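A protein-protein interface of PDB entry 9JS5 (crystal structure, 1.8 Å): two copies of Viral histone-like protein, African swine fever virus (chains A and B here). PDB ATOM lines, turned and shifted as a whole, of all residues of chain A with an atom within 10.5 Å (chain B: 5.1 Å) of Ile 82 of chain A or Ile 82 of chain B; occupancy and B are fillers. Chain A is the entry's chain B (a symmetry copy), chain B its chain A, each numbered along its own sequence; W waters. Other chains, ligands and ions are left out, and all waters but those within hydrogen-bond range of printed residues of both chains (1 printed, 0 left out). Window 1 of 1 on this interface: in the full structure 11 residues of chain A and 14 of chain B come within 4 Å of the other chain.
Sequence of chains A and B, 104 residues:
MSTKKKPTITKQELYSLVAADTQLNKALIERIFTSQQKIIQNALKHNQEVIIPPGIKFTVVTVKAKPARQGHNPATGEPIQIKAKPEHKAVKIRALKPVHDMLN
Of the 18 printed residues of chain A, 9 touch a printed residue of chain B.
Hydrophobic or aromatic side chains of chain A within 4 Å of the printed part of chain B: Pro 67, Ile 80 and Ile 82.
Of the 10 printed residues of chain B, 9 touch a printed residue of chain A.
Hydrophobic or aromatic side chains of chain B that line the printed part of chain A: Pro 67, Ile 80 and Ile 82.
Among the printed residues, 20 pairs touch across the chains.
Among the printed residues, no Asp or Glu carboxylate lies within 4 Å of a Lys or Arg side-chain nitrogen of the other chain.
Pro 67 of chain A touches its own counterpart, Pro 67 of chain B.
Arg 69 of chain A touches Ala 84 of chain B, but with the chains exchanged Ala 84 of chain A does not touch Arg 69 of chain B (4.1 Å).
Ile 80 of chain B touches its own counterpart, Ile 80 of chain A.
Ile 82 of chain A touches Gln 70 of chain B, but with the chains exchanged Gln 70 of chain A does not touch Ile 82 of chain B (4.1 Å).
10 positions are printed for both chains.
Of the 20 pairs that touch across the chains among the printed residues, 12 have their exchanged pair printed and touching as well.
The backbone carbonyl oxygen (O) of Lys 83 of chain B sits at hydrogen-bond distance from the guanidinium group (NH2) of Arg 69 of chain A (2.5 Å).
NZ of Lys 66 of chain A sits at hydrogen-bond distance from O of Ala 68 of chain B (2.9 Å).
The guanidinium group (NH1) of Arg 69 of chain B sits at hydrogen-bond distance from the backbone carbonyl oxygen (O) of Pro 67 of chain A (2.9 Å).
O of Pro 67 of chain B lies within hydrogen-bond range of NH2 of Arg 69 of chain A, 3.0 Å away.
The backbone carbonyl oxygen of Lys 83 of chain A is in hydrogen-bond range of the guanidinium group of Arg 69 of chain B (3.0 Å).
Water W1 lies within hydrogen-bond range of the backbone carbonyl oxygen (O) of Gln 81 of chain B (2.9 Å) and the backbone NH (N) of His 72 of chain A (3.1 Å).
O of Arg 69 of chain B is in hydrogen-bond range of N of Ile 82 of chain B (2.9 Å).
N of Gly 71 of chain B lies within hydrogen-bond range of O of Ile 80 of chain B (2.8 Å).
O of Arg 69 of chain A sits at hydrogen-bond distance from N of Ile 82 of chain A, 2.9 Å away.
The backbone NH of Gly 71 of chain A lies within hydrogen-bond range of the backbone carbonyl oxygen of Ile 80 of chain A, at 2.6 Å.
NE2 of Gln 81 of chain A lies within hydrogen-bond range of O of Arg 69 of chain A.
The backbone NH of Lys 85 of chain A is in hydrogen-bond range of the backbone carbonyl oxygen of Lys 66 of chain A.
Among the printed residues, pairs that only touch across the chains: Gly 71 of chain A with Ile 82 of chain B, Arg 69 of chain A with Ile 82 of chain B, Ile 82 of chain A with Ile 82 of chain B, Lys 66 of chain A with Arg 69 of chain B, Ile 82 of chain A with Ile 80 of chain B, Ile 82 of chain A with Gln 70 of chain B, Ile 80 of chain A with Ile 80 of chain B, Ile 82 of chain A with Arg 69 of chain B, Arg 69 of chain A with Ala 84 of chain B, Pro 67 of chain A with Pro 67 of chain B, Ile 82 of chain A with Gly 71 of chain B, His 72 of chain A with Ile 80 of chain B, Lys 85 of chain A with Arg 69 of chain B, Arg 69 of chain A with Arg 69 of chain B and Lys 66 of chain A with Pro 67 of chain B.
Of the printed residues of chain B, Lys 66 of chain A touches Pro 67 (3.9 Å), Ala 68 (2.9 Å) and Arg 69 (3.6 Å).
Glu 78 of chain A touches none of the printed residues of chain B.
Pro 79 of chain A touches none of the printed residues of chain B.
Ile 82 of chain A touches five residues of chain B.
Of the printed residues of chain A, Pro 67 of chain B touches Lys 66, Pro 67 and Arg 69.
Printed residues of chain A within 4 Å of Ala 68 of chain B: Lys 66 (2.9 Å).
Arg 69 of chain B touches six residues of chain A.
Gly 71 of chain B touches just one residue of chain A: Ile 82.
Of the printed residues of chain A, Ile 80 of chain B touches His 72, Ile 80 and Ile 82.
Ile 82 of chain B touches three residues of chain A.
Lys 83 of chain B touches one residue of chain A.
Of chain A, only Arg 69 comes within 4 Å of Ala 84 of chain B.
The nearest printed residue of chain B that does not touch Pro 67 of chain A is Ala 68 of chain B (6.7 Å).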
ATOM      1  N   LYS A  66       0.529  10.791 -10.419  1.00  0.00           N
ATOM      2  CA  LYS A  66       0.628   9.658  -9.510  1.00  0.00           C
ATOM      3  C   LYS A  66       1.184  10.142  -8.180  1.00  0.00           C
ATOM      4  O   LYS A  66       2.065  11.013  -8.149  1.00  0.00           O
ATOM      5  CB  LYS A  66       1.504   8.541 -10.081  1.00  0.00           C
ATOM      6  CG  LYS A  66       1.009   8.012 -11.448  1.00  0.00           C
ATOM      7  CD  LYS A  66       0.176   6.737 -11.312  1.00  0.00           C
ATOM      8  CE  LYS A  66       0.446   5.754 -12.479  1.00  0.00           C
ATOM      9  NZ  LYS A  66       0.919   4.395 -11.997  1.00  0.00           N
ATOM     10  N   PRO A  67       0.685   9.605  -7.075  1.00  0.00           N
ATOM     11  CA  PRO A  67       1.105  10.085  -5.758  1.00  0.00           C
ATOM     12  C   PRO A  67       2.429   9.470  -5.331  1.00  0.00           C
ATOM     13  O   PRO A  67       2.841   8.413  -5.807  1.00  0.00           O
ATOM     14  CB  PRO A  67      -0.036   9.623  -4.849  1.00  0.00           C
ATOM     15  CG  PRO A  67      -0.505   8.357  -5.488  1.00  0.00           C
ATOM     16  CD  PRO A  67      -0.386   8.598  -6.983  1.00  0.00           C
ATOM     17  N   ALA A  68       3.088  10.156  -4.400  1.00  0.00           N
ATOM     18  CA  ALA A  68       4.291   9.618  -3.785  1.00  0.00           C
ATOM     19  C   ALA A  68       3.976   8.330  -3.030  1.00  0.00           C
ATOM     20  O   ALA A  68       2.890   8.155  -2.477  1.00  0.00           O
ATOM     21  CB  ALA A  68       4.904  10.632  -2.820  1.00  0.00           C
ATOM     22  N   ARG A  69       4.945   7.419  -3.011  1.00  0.00           N
ATOM     23  CA  ARG A  69       4.813   6.148  -2.306  1.00  0.00           C
ATOM     24  C   ARG A  69       6.177   5.774  -1.747  1.00  0.00           C
ATOM     25  O   ARG A  69       7.201   6.110  -2.344  1.00  0.00           O
ATOM     26  CB  ARG A  69       4.299   5.045  -3.243  1.00  0.00           C
ATOM     27  CG  ARG A  69       2.859   5.222  -3.748  1.00  0.00           C
ATOM     28  CD  ARG A  69       1.997   4.165  -3.128  1.00  0.00           C
ATOM     29  NE  ARG A  69       1.747   3.074  -4.052  1.00  0.00           N
ATOM     30  CZ  ARG A  69       1.558   1.818  -3.673  1.00  0.00           C
ATOM     31  NH1 ARG A  69       1.639   1.456  -2.402  1.00  0.00           N
ATOM     32  NH2 ARG A  69       1.293   0.899  -4.596  1.00  0.00           N
ATOM     33  N   GLN A  70       6.221   5.091  -0.607  1.00  0.00           N
ATOM     34  CA  GLN A  70       7.534   4.755  -0.064  1.00  0.00           C
ATOM     35  C   GLN A  70       7.924   3.355  -0.512  1.00  0.00           C
ATOM     36  O   GLN A  70       7.158   2.396  -0.352  1.00  0.00           O
ATOM     37  CB  GLN A  70       7.605   4.895   1.455  1.00  0.00           C
ATOM     38  CG  GLN A  70       8.989   4.465   2.002  1.00  0.00           C
ATOM     39  CD  GLN A  70       9.554   5.458   3.007  1.00  0.00           C
ATOM     40  OE1 GLN A  70       9.015   5.623   4.096  1.00  0.00           O
ATOM     41  NE2 GLN A  70      10.668   6.112   2.642  1.00  0.00           N
ATOM     42  N   GLY A  71       9.097   3.257  -1.122  1.00  0.00           N
ATOM     43  CA  GLY A  71       9.641   1.996  -1.559  1.00  0.00           C
ATOM     44  C   GLY A  71      10.739   1.526  -0.632  1.00  0.00           C
ATOM     45  O   GLY A  71      10.978   2.093   0.434  1.00  0.00           O
ATOM     46  N   HIS A  72      11.386   0.441  -1.042  1.00  0.00           N
ATOM     47  CA  HIS A  72      12.502  -0.099  -0.287  1.00  0.00           C
ATOM     48  C   HIS A  72      13.510  -0.713  -1.241  1.00  0.00           C
ATOM     49  O   HIS A  72      13.141  -1.255  -2.291  1.00  0.00           O
ATOM     50  CB  HIS A  72      12.057  -1.168   0.729  1.00  0.00           C
ATOM     51  CG  HIS A  72      11.176  -0.637   1.817  1.00  0.00           C
ATOM     52  ND1 HIS A  72       9.838  -0.360   1.620  1.00  0.00           N
ATOM     53  CD2 HIS A  72      11.455  -0.273   3.090  1.00  0.00           C
ATOM     54  CE1 HIS A  72       9.323   0.111   2.742  1.00  0.00           C
ATOM     55  NE2 HIS A  72      10.283   0.174   3.649  1.00  0.00           N
ATOM     56  N   ASN A  73      14.781  -0.620  -0.871  1.00  0.00           N
ATOM     57  CA  ASN A  73      15.795  -1.516  -1.429  1.00  0.00           C
ATOM     58  C   ASN A  73      15.402  -2.941  -1.059  1.00  0.00           C
ATOM     59  O   ASN A  73      15.389  -3.290   0.125  1.00  0.00           O
ATOM     60  CB  ASN A  73      17.177  -1.135  -0.883  1.00  0.00           C
ATOM     61  CG  ASN A  73      18.295  -1.989  -1.440  1.00  0.00           C
ATOM     62  OD1 ASN A  73      18.082  -3.133  -1.821  1.00  0.00           O
ATOM     63  ND2 ASN A  73      19.502  -1.411  -1.519  1.00  0.00           N
ATOM     64  N   PRO A  74      15.063  -3.797  -2.027  1.00  0.00           N
ATOM     65  CA  PRO A  74      14.521  -5.121  -1.659  1.00  0.00           C
ATOM     66  C   PRO A  74      15.565  -6.061  -1.065  1.00  0.00           C
ATOM     67  O   PRO A  74      15.189  -7.038  -0.397  1.00  0.00           O
ATOM     68  CB  PRO A  74      13.968  -5.654  -2.990  1.00  0.00           C
ATOM     69  CG  PRO A  74      14.814  -4.998  -4.018  1.00  0.00           C
ATOM     70  CD  PRO A  74      15.100  -3.595  -3.485  1.00  0.00           C
ATOM     71  N   GLU A  78      16.415  -0.797   2.988  1.00  0.00           N
ATOM     72  CA  GLU A  78      16.536   0.653   2.989  1.00  0.00           C
ATOM     73  C   GLU A  78      15.261   1.290   2.459  1.00  0.00           C
ATOM     74  O   GLU A  78      14.813   0.945   1.358  1.00  0.00           O
ATOM     75  CB  GLU A  78      17.723   1.092   2.134  1.00  0.00           C
ATOM     76  CG  GLU A  78      17.922   2.620   2.084  1.00  0.00           C
ATOM     77  CD  GLU A  78      18.778   3.025   0.896  1.00  0.00           C
ATOM     78  OE1 GLU A  78      18.950   2.175  -0.006  1.00  0.00           O
ATOM     79  OE2 GLU A  78      19.279   4.179   0.876  1.00  0.00           O
ATOM     80  N   PRO A  79      14.649   2.211   3.202  1.00  0.00           N
ATOM     81  CA  PRO A  79      13.519   2.982   2.654  1.00  0.00           C
ATOM     82  C   PRO A  79      13.961   3.920   1.536  1.00  0.00           C
ATOM     83  O   PRO A  79      14.962   4.627   1.653  1.00  0.00           O
ATOM     84  CB  PRO A  79      12.978   3.752   3.870  1.00  0.00           C
ATOM     85  CG  PRO A  79      13.917   3.493   5.003  1.00  0.00           C
ATOM     86  CD  PRO A  79      15.042   2.624   4.561  1.00  0.00           C
ATOM     87  N   ILE A  80      13.208   3.919   0.434  1.00  0.00           N
ATOM     88  CA  ILE A  80      13.486   4.778  -0.707  1.00  0.00           C
ATOM     89  C   ILE A  80      12.181   5.458  -1.104  1.00  0.00           C
ATOM     90  O   ILE A  80      11.216   4.790  -1.489  1.00  0.00           O
ATOM     91  CB  ILE A  80      14.088   4.004  -1.894  1.00  0.00           C
ATOM     92  CG1 ILE A  80      15.484   3.505  -1.531  1.00  0.00           C
ATOM     93  CG2 ILE A  80      14.221   4.901  -3.118  1.00  0.00           C
ATOM     94  CD1 ILE A  80      16.047   2.482  -2.504  1.00  0.00           C
ATOM     95  N   GLN A  81      12.146   6.776  -0.976  1.00  0.00           N
ATOM     96  CA  GLN A  81      10.985   7.556  -1.376  1.00  0.00           C
ATOM     97  C   GLN A  81      10.845   7.555  -2.892  1.00  0.00           C
ATOM     98  O   GLN A  81      11.816   7.786  -3.621  1.00  0.00           O
ATOM     99  CB  GLN A  81      11.122   8.993  -0.863  1.00  0.00           C
ATOM    100  CG  GLN A  81       9.815   9.755  -0.698  1.00  0.00           C
ATOM    101  CD  GLN A  81       8.704   8.925  -0.087  1.00  0.00           C
ATOM    102  OE1 GLN A  81       8.913   8.209   0.896  1.00  0.00           O
ATOM    103  NE2 GLN A  81       7.514   9.008  -0.677  1.00  0.00           N
ATOM    104  N   ILE A  82       9.636   7.301  -3.375  1.00  0.00           N
ATOM    105  CA  ILE A  82       9.327   7.480  -4.787  1.00  0.00           C
ATOM    106  C   ILE A  82       8.444   8.711  -4.878  1.00  0.00           C
ATOM    107  O   ILE A  82       7.291   8.682  -4.437  1.00  0.00           O
ATOM    108  CB  ILE A  82       8.639   6.252  -5.387  1.00  0.00           C
ATOM    109  CG1 ILE A  82       9.629   5.102  -5.471  1.00  0.00           C
ATOM    110  CG2 ILE A  82       8.150   6.567  -6.785  1.00  0.00           C
ATOM    111  CD1 ILE A  82       8.984   3.814  -5.838  1.00  0.00           C
ATOM    112  N   LYS A  83       8.990   9.798  -5.422  1.00  0.00           N
ATOM    113  CA  LYS A  83       8.310  11.084  -5.379  1.00  0.00           C
ATOM    114  C   LYS A  83       7.038  11.055  -6.212  1.00  0.00           C
ATOM    115  O   LYS A  83       6.863  10.228  -7.114  1.00  0.00           O
ATOM    116  CB  LYS A  83       9.223  12.203  -5.880  1.00  0.00           C
ATOM    117  CG  LYS A  83      10.260  12.692  -4.870  1.00  0.00           C
ATOM    118  CD  LYS A  83      11.672  12.650  -5.447  1.00  0.00           C
ATOM    119  CE  LYS A  83      12.708  13.116  -4.429  1.00  0.00           C
ATOM    120  NZ  LYS A  83      13.731  14.027  -5.045  1.00  0.00           N
ATOM    121  N   ALA A  84       6.134  11.974  -5.890  1.00  0.00           N
ATOM    122  CA  ALA A  84       4.918  12.103  -6.677  1.00  0.00           C
ATOM    123  C   ALA A  84       5.261  12.538  -8.093  1.00  0.00           C
ATOM    124  O   ALA A  84       6.280  13.193  -8.337  1.00  0.00           O
ATOM    125  CB  ALA A  84       3.964  13.106  -6.038  1.00  0.00           C
ATOM    126  N   LYS A  85       4.404  12.155  -9.033  1.00  0.00           N
ATOM    127  CA  LYS A  85       4.622  12.490 -10.430  1.00  0.00           C
ATOM    128  C   LYS A  85       3.473  13.364 -10.912  1.00  0.00           C
ATOM    129  O   LYS A  85       2.304  12.945 -10.858  1.00  0.00           O
ATOM    130  CB  LYS A  85       4.757  11.216 -11.281  1.00  0.00           C
ATOM    131  CG  LYS A  85       4.015  11.186 -12.612  1.00  0.00           C
ATOM    132  CD  LYS A  85       4.513  10.077 -13.536  1.00  0.00           C
ATOM    133  CE  LYS A  85       3.699   8.787 -13.402  1.00  0.00           C
ATOM    134  NZ  LYS A  85       3.929   7.811 -14.538  1.00  0.00           N
ATOM    135  N   PRO A  86       3.756  14.580 -11.363  1.00  0.00           N
ATOM    136  CA  PRO A  86       2.692  15.468 -11.830  1.00  0.00           C
ATOM    137  C   PRO A  86       2.094  14.977 -13.138  1.00  0.00           C
ATOM    138  O   PRO A  86       2.737  14.289 -13.934  1.00  0.00           O
ATOM    139  CB  PRO A  86       3.426  16.795 -12.054  1.00  0.00           C
ATOM    140  CG  PRO A  86       4.781  16.337 -12.533  1.00  0.00           C
ATOM    141  CD  PRO A  86       5.092  15.140 -11.641  1.00  0.00           C
ATOM    142  N   PRO B  67      -2.001   3.339  -6.734  1.00  0.00           N
ATOM    143  CA  PRO B  67      -1.473   2.737  -7.954  1.00  0.00           C
ATOM    144  C   PRO B  67      -0.043   2.253  -7.780  1.00  0.00           C
ATOM    145  O   PRO B  67       0.697   2.703  -6.899  1.00  0.00           O
ATOM    146  CB  PRO B  67      -1.555   3.885  -8.964  1.00  0.00           C
ATOM    147  CG  PRO B  67      -1.308   5.101  -8.104  1.00  0.00           C
ATOM    148  CD  PRO B  67      -1.987   4.813  -6.794  1.00  0.00           C
ATOM    149  N   ALA B  68       0.334   1.309  -8.636  1.00  0.00           N
ATOM    150  CA  ALA B  68       1.720   0.875  -8.714  1.00  0.00           C
ATOM    151  C   ALA B  68       2.620   2.053  -9.071  1.00  0.00           C
ATOM    152  O   ALA B  68       2.211   2.986  -9.768  1.00  0.00           O
ATOM    153  CB  ALA B  68       1.866  -0.232  -9.761  1.00  0.00           C
ATOM    154  N   ARG B  69       3.858   2.019  -8.575  1.00  0.00           N
ATOM    155  CA  ARG B  69       4.846   3.031  -8.918  1.00  0.00           C
ATOM    156  C   ARG B  69       6.180   2.380  -9.228  1.00  0.00           C
ATOM    157  O   ARG B  69       6.507   1.315  -8.703  1.00  0.00           O
ATOM    158  CB  ARG B  69       5.065   4.065  -7.780  1.00  0.00           C
ATOM    159  CG  ARG B  69       3.868   4.969  -7.458  1.00  0.00           C
ATOM    160  CD  ARG B  69       3.420   5.805  -8.665  1.00  0.00           C
ATOM    161  NE  ARG B  69       4.513   6.427  -9.403  1.00  0.00           N
ATOM    162  CZ  ARG B  69       5.186   7.506  -9.018  1.00  0.00           C
ATOM    163  NH1 ARG B  69       4.905   8.134  -7.887  1.00  0.00           N
ATOM    164  NH2 ARG B  69       6.162   7.968  -9.793  1.00  0.00           N
ATOM    165  N   GLN B  70       6.953   3.058 -10.067  1.00  0.00           N
ATOM    166  CA  GLN B  70       8.324   2.685 -10.368  1.00  0.00           C
ATOM    167  C   GLN B  70       9.222   3.832  -9.936  1.00  0.00           C
ATOM    168  O   GLN B  70       8.871   5.008 -10.101  1.00  0.00           O
ATOM    169  CB  GLN B  70       8.530   2.423 -11.864  1.00  0.00           C
ATOM    170  CG  GLN B  70       7.619   1.356 -12.465  1.00  0.00           C
ATOM    171  CD  GLN B  70       7.662   1.348 -13.993  1.00  0.00           C
ATOM    172  OE1 GLN B  70       8.716   1.141 -14.588  1.00  0.00           O
ATOM    173  NE2 GLN B  70       6.515   1.592 -14.627  1.00  0.00           N
ATOM    174  N   GLY B  71      10.367   3.493  -9.365  1.00  0.00           N
ATOM    175  CA  GLY B  71      11.347   4.507  -9.045  1.00  0.00           C
ATOM    176  C   GLY B  71      12.748   3.966  -9.201  1.00  0.00           C
ATOM    177  O   GLY B  71      12.962   2.969  -9.901  1.00  0.00           O
ATOM    178  N   ILE B  80      13.352   0.287  -8.658  1.00  0.00           N
ATOM    179  CA  ILE B  80      12.561  -0.326  -7.602  1.00  0.00           C
ATOM    180  C   ILE B  80      11.097  -0.140  -7.964  1.00  0.00           C
ATOM    181  O   ILE B  80      10.732   0.781  -8.702  1.00  0.00           O
ATOM    182  CB  ILE B  80      12.861   0.264  -6.210  1.00  0.00           C
ATOM    183  CG1 ILE B  80      12.621   1.773  -6.214  1.00  0.00           C
ATOM    184  CG2 ILE B  80      14.266  -0.079  -5.759  1.00  0.00           C
ATOM    185  CD1 ILE B  80      12.198   2.292  -4.866  1.00  0.00           C
ATOM    186  N   GLN B  81      10.259  -1.032  -7.452  1.00  0.00           N
ATOM    187  CA  GLN B  81       8.846  -1.055  -7.815  1.00  0.00           C
ATOM    188  C   GLN B  81       7.992  -1.212  -6.572  1.00  0.00           C
ATOM    189  O   GLN B  81       8.401  -1.865  -5.604  1.00  0.00           O
ATOM    190  CB  GLN B  81       8.523  -2.192  -8.791  1.00  0.00           C
ATOM    191  CG  GLN B  81       9.106  -2.001 -10.190  1.00  0.00           C
ATOM    192  CD  GLN B  81      10.549  -2.463 -10.319  1.00  0.00           C
ATOM    193  OE1 GLN B  81      11.083  -3.139  -9.433  1.00  0.00           O
ATOM    194  NE2 GLN B  81      11.200  -2.071 -11.412  1.00  0.00           N
ATOM    195  N   ILE B  82       6.810  -0.598  -6.605  1.00  0.00           N
ATOM    196  CA  ILE B  82       5.763  -0.775  -5.600  1.00  0.00           C
ATOM    197  C   ILE B  82       4.552  -1.333  -6.330  1.00  0.00           C
ATOM    198  O   ILE B  82       4.079  -0.718  -7.294  1.00  0.00           O
ATOM    199  CB  ILE B  82       5.369   0.540  -4.902  1.00  0.00           C
ATOM    200  CG1 ILE B  82       6.538   1.504  -4.718  1.00  0.00           C
ATOM    201  CG2 ILE B  82       4.737   0.242  -3.547  1.00  0.00           C
ATOM    202  CD1 ILE B  82       7.750   0.913  -4.126  1.00  0.00           C
ATOM    203  N   LYS B  83       4.051  -2.484  -5.889  1.00  0.00           N
ATOM    204  CA  LYS B  83       2.851  -3.037  -6.506  1.00  0.00           C
ATOM    205  C   LYS B  83       1.640  -2.183  -6.161  1.00  0.00           C
ATOM    206  O   LYS B  83       1.601  -1.505  -5.128  1.00  0.00           O
ATOM    207  CB  LYS B  83       2.579  -4.483  -6.062  1.00  0.00           C
ATOM    208  CG  LYS B  83       3.610  -5.551  -6.475  1.00  0.00           C
ATOM    209  CD  LYS B  83       4.736  -5.639  -5.466  1.00  0.00           C
ATOM    210  CE  LYS B  83       5.300  -7.052  -5.251  1.00  0.00           C
ATOM    211  NZ  LYS B  83       6.744  -6.978  -4.799  1.00  0.00           N
ATOM    212  N   ALA B  84       0.647  -2.219  -7.043  1.00  0.00           N
ATOM    213  CA  ALA B  84      -0.609  -1.544  -6.775  1.00  0.00           C
ATOM    214  C   ALA B  84      -1.273  -2.144  -5.544  1.00  0.00           C
ATOM    215  O   ALA B  84      -1.194  -3.350  -5.293  1.00  0.00           O
ATOM    216  CB  ALA B  84      -1.538  -1.649  -7.982  1.00  0.00           C
HETATM  217  O   HOH W   1       9.864  -1.199  -3.160  1.00  0.00           O
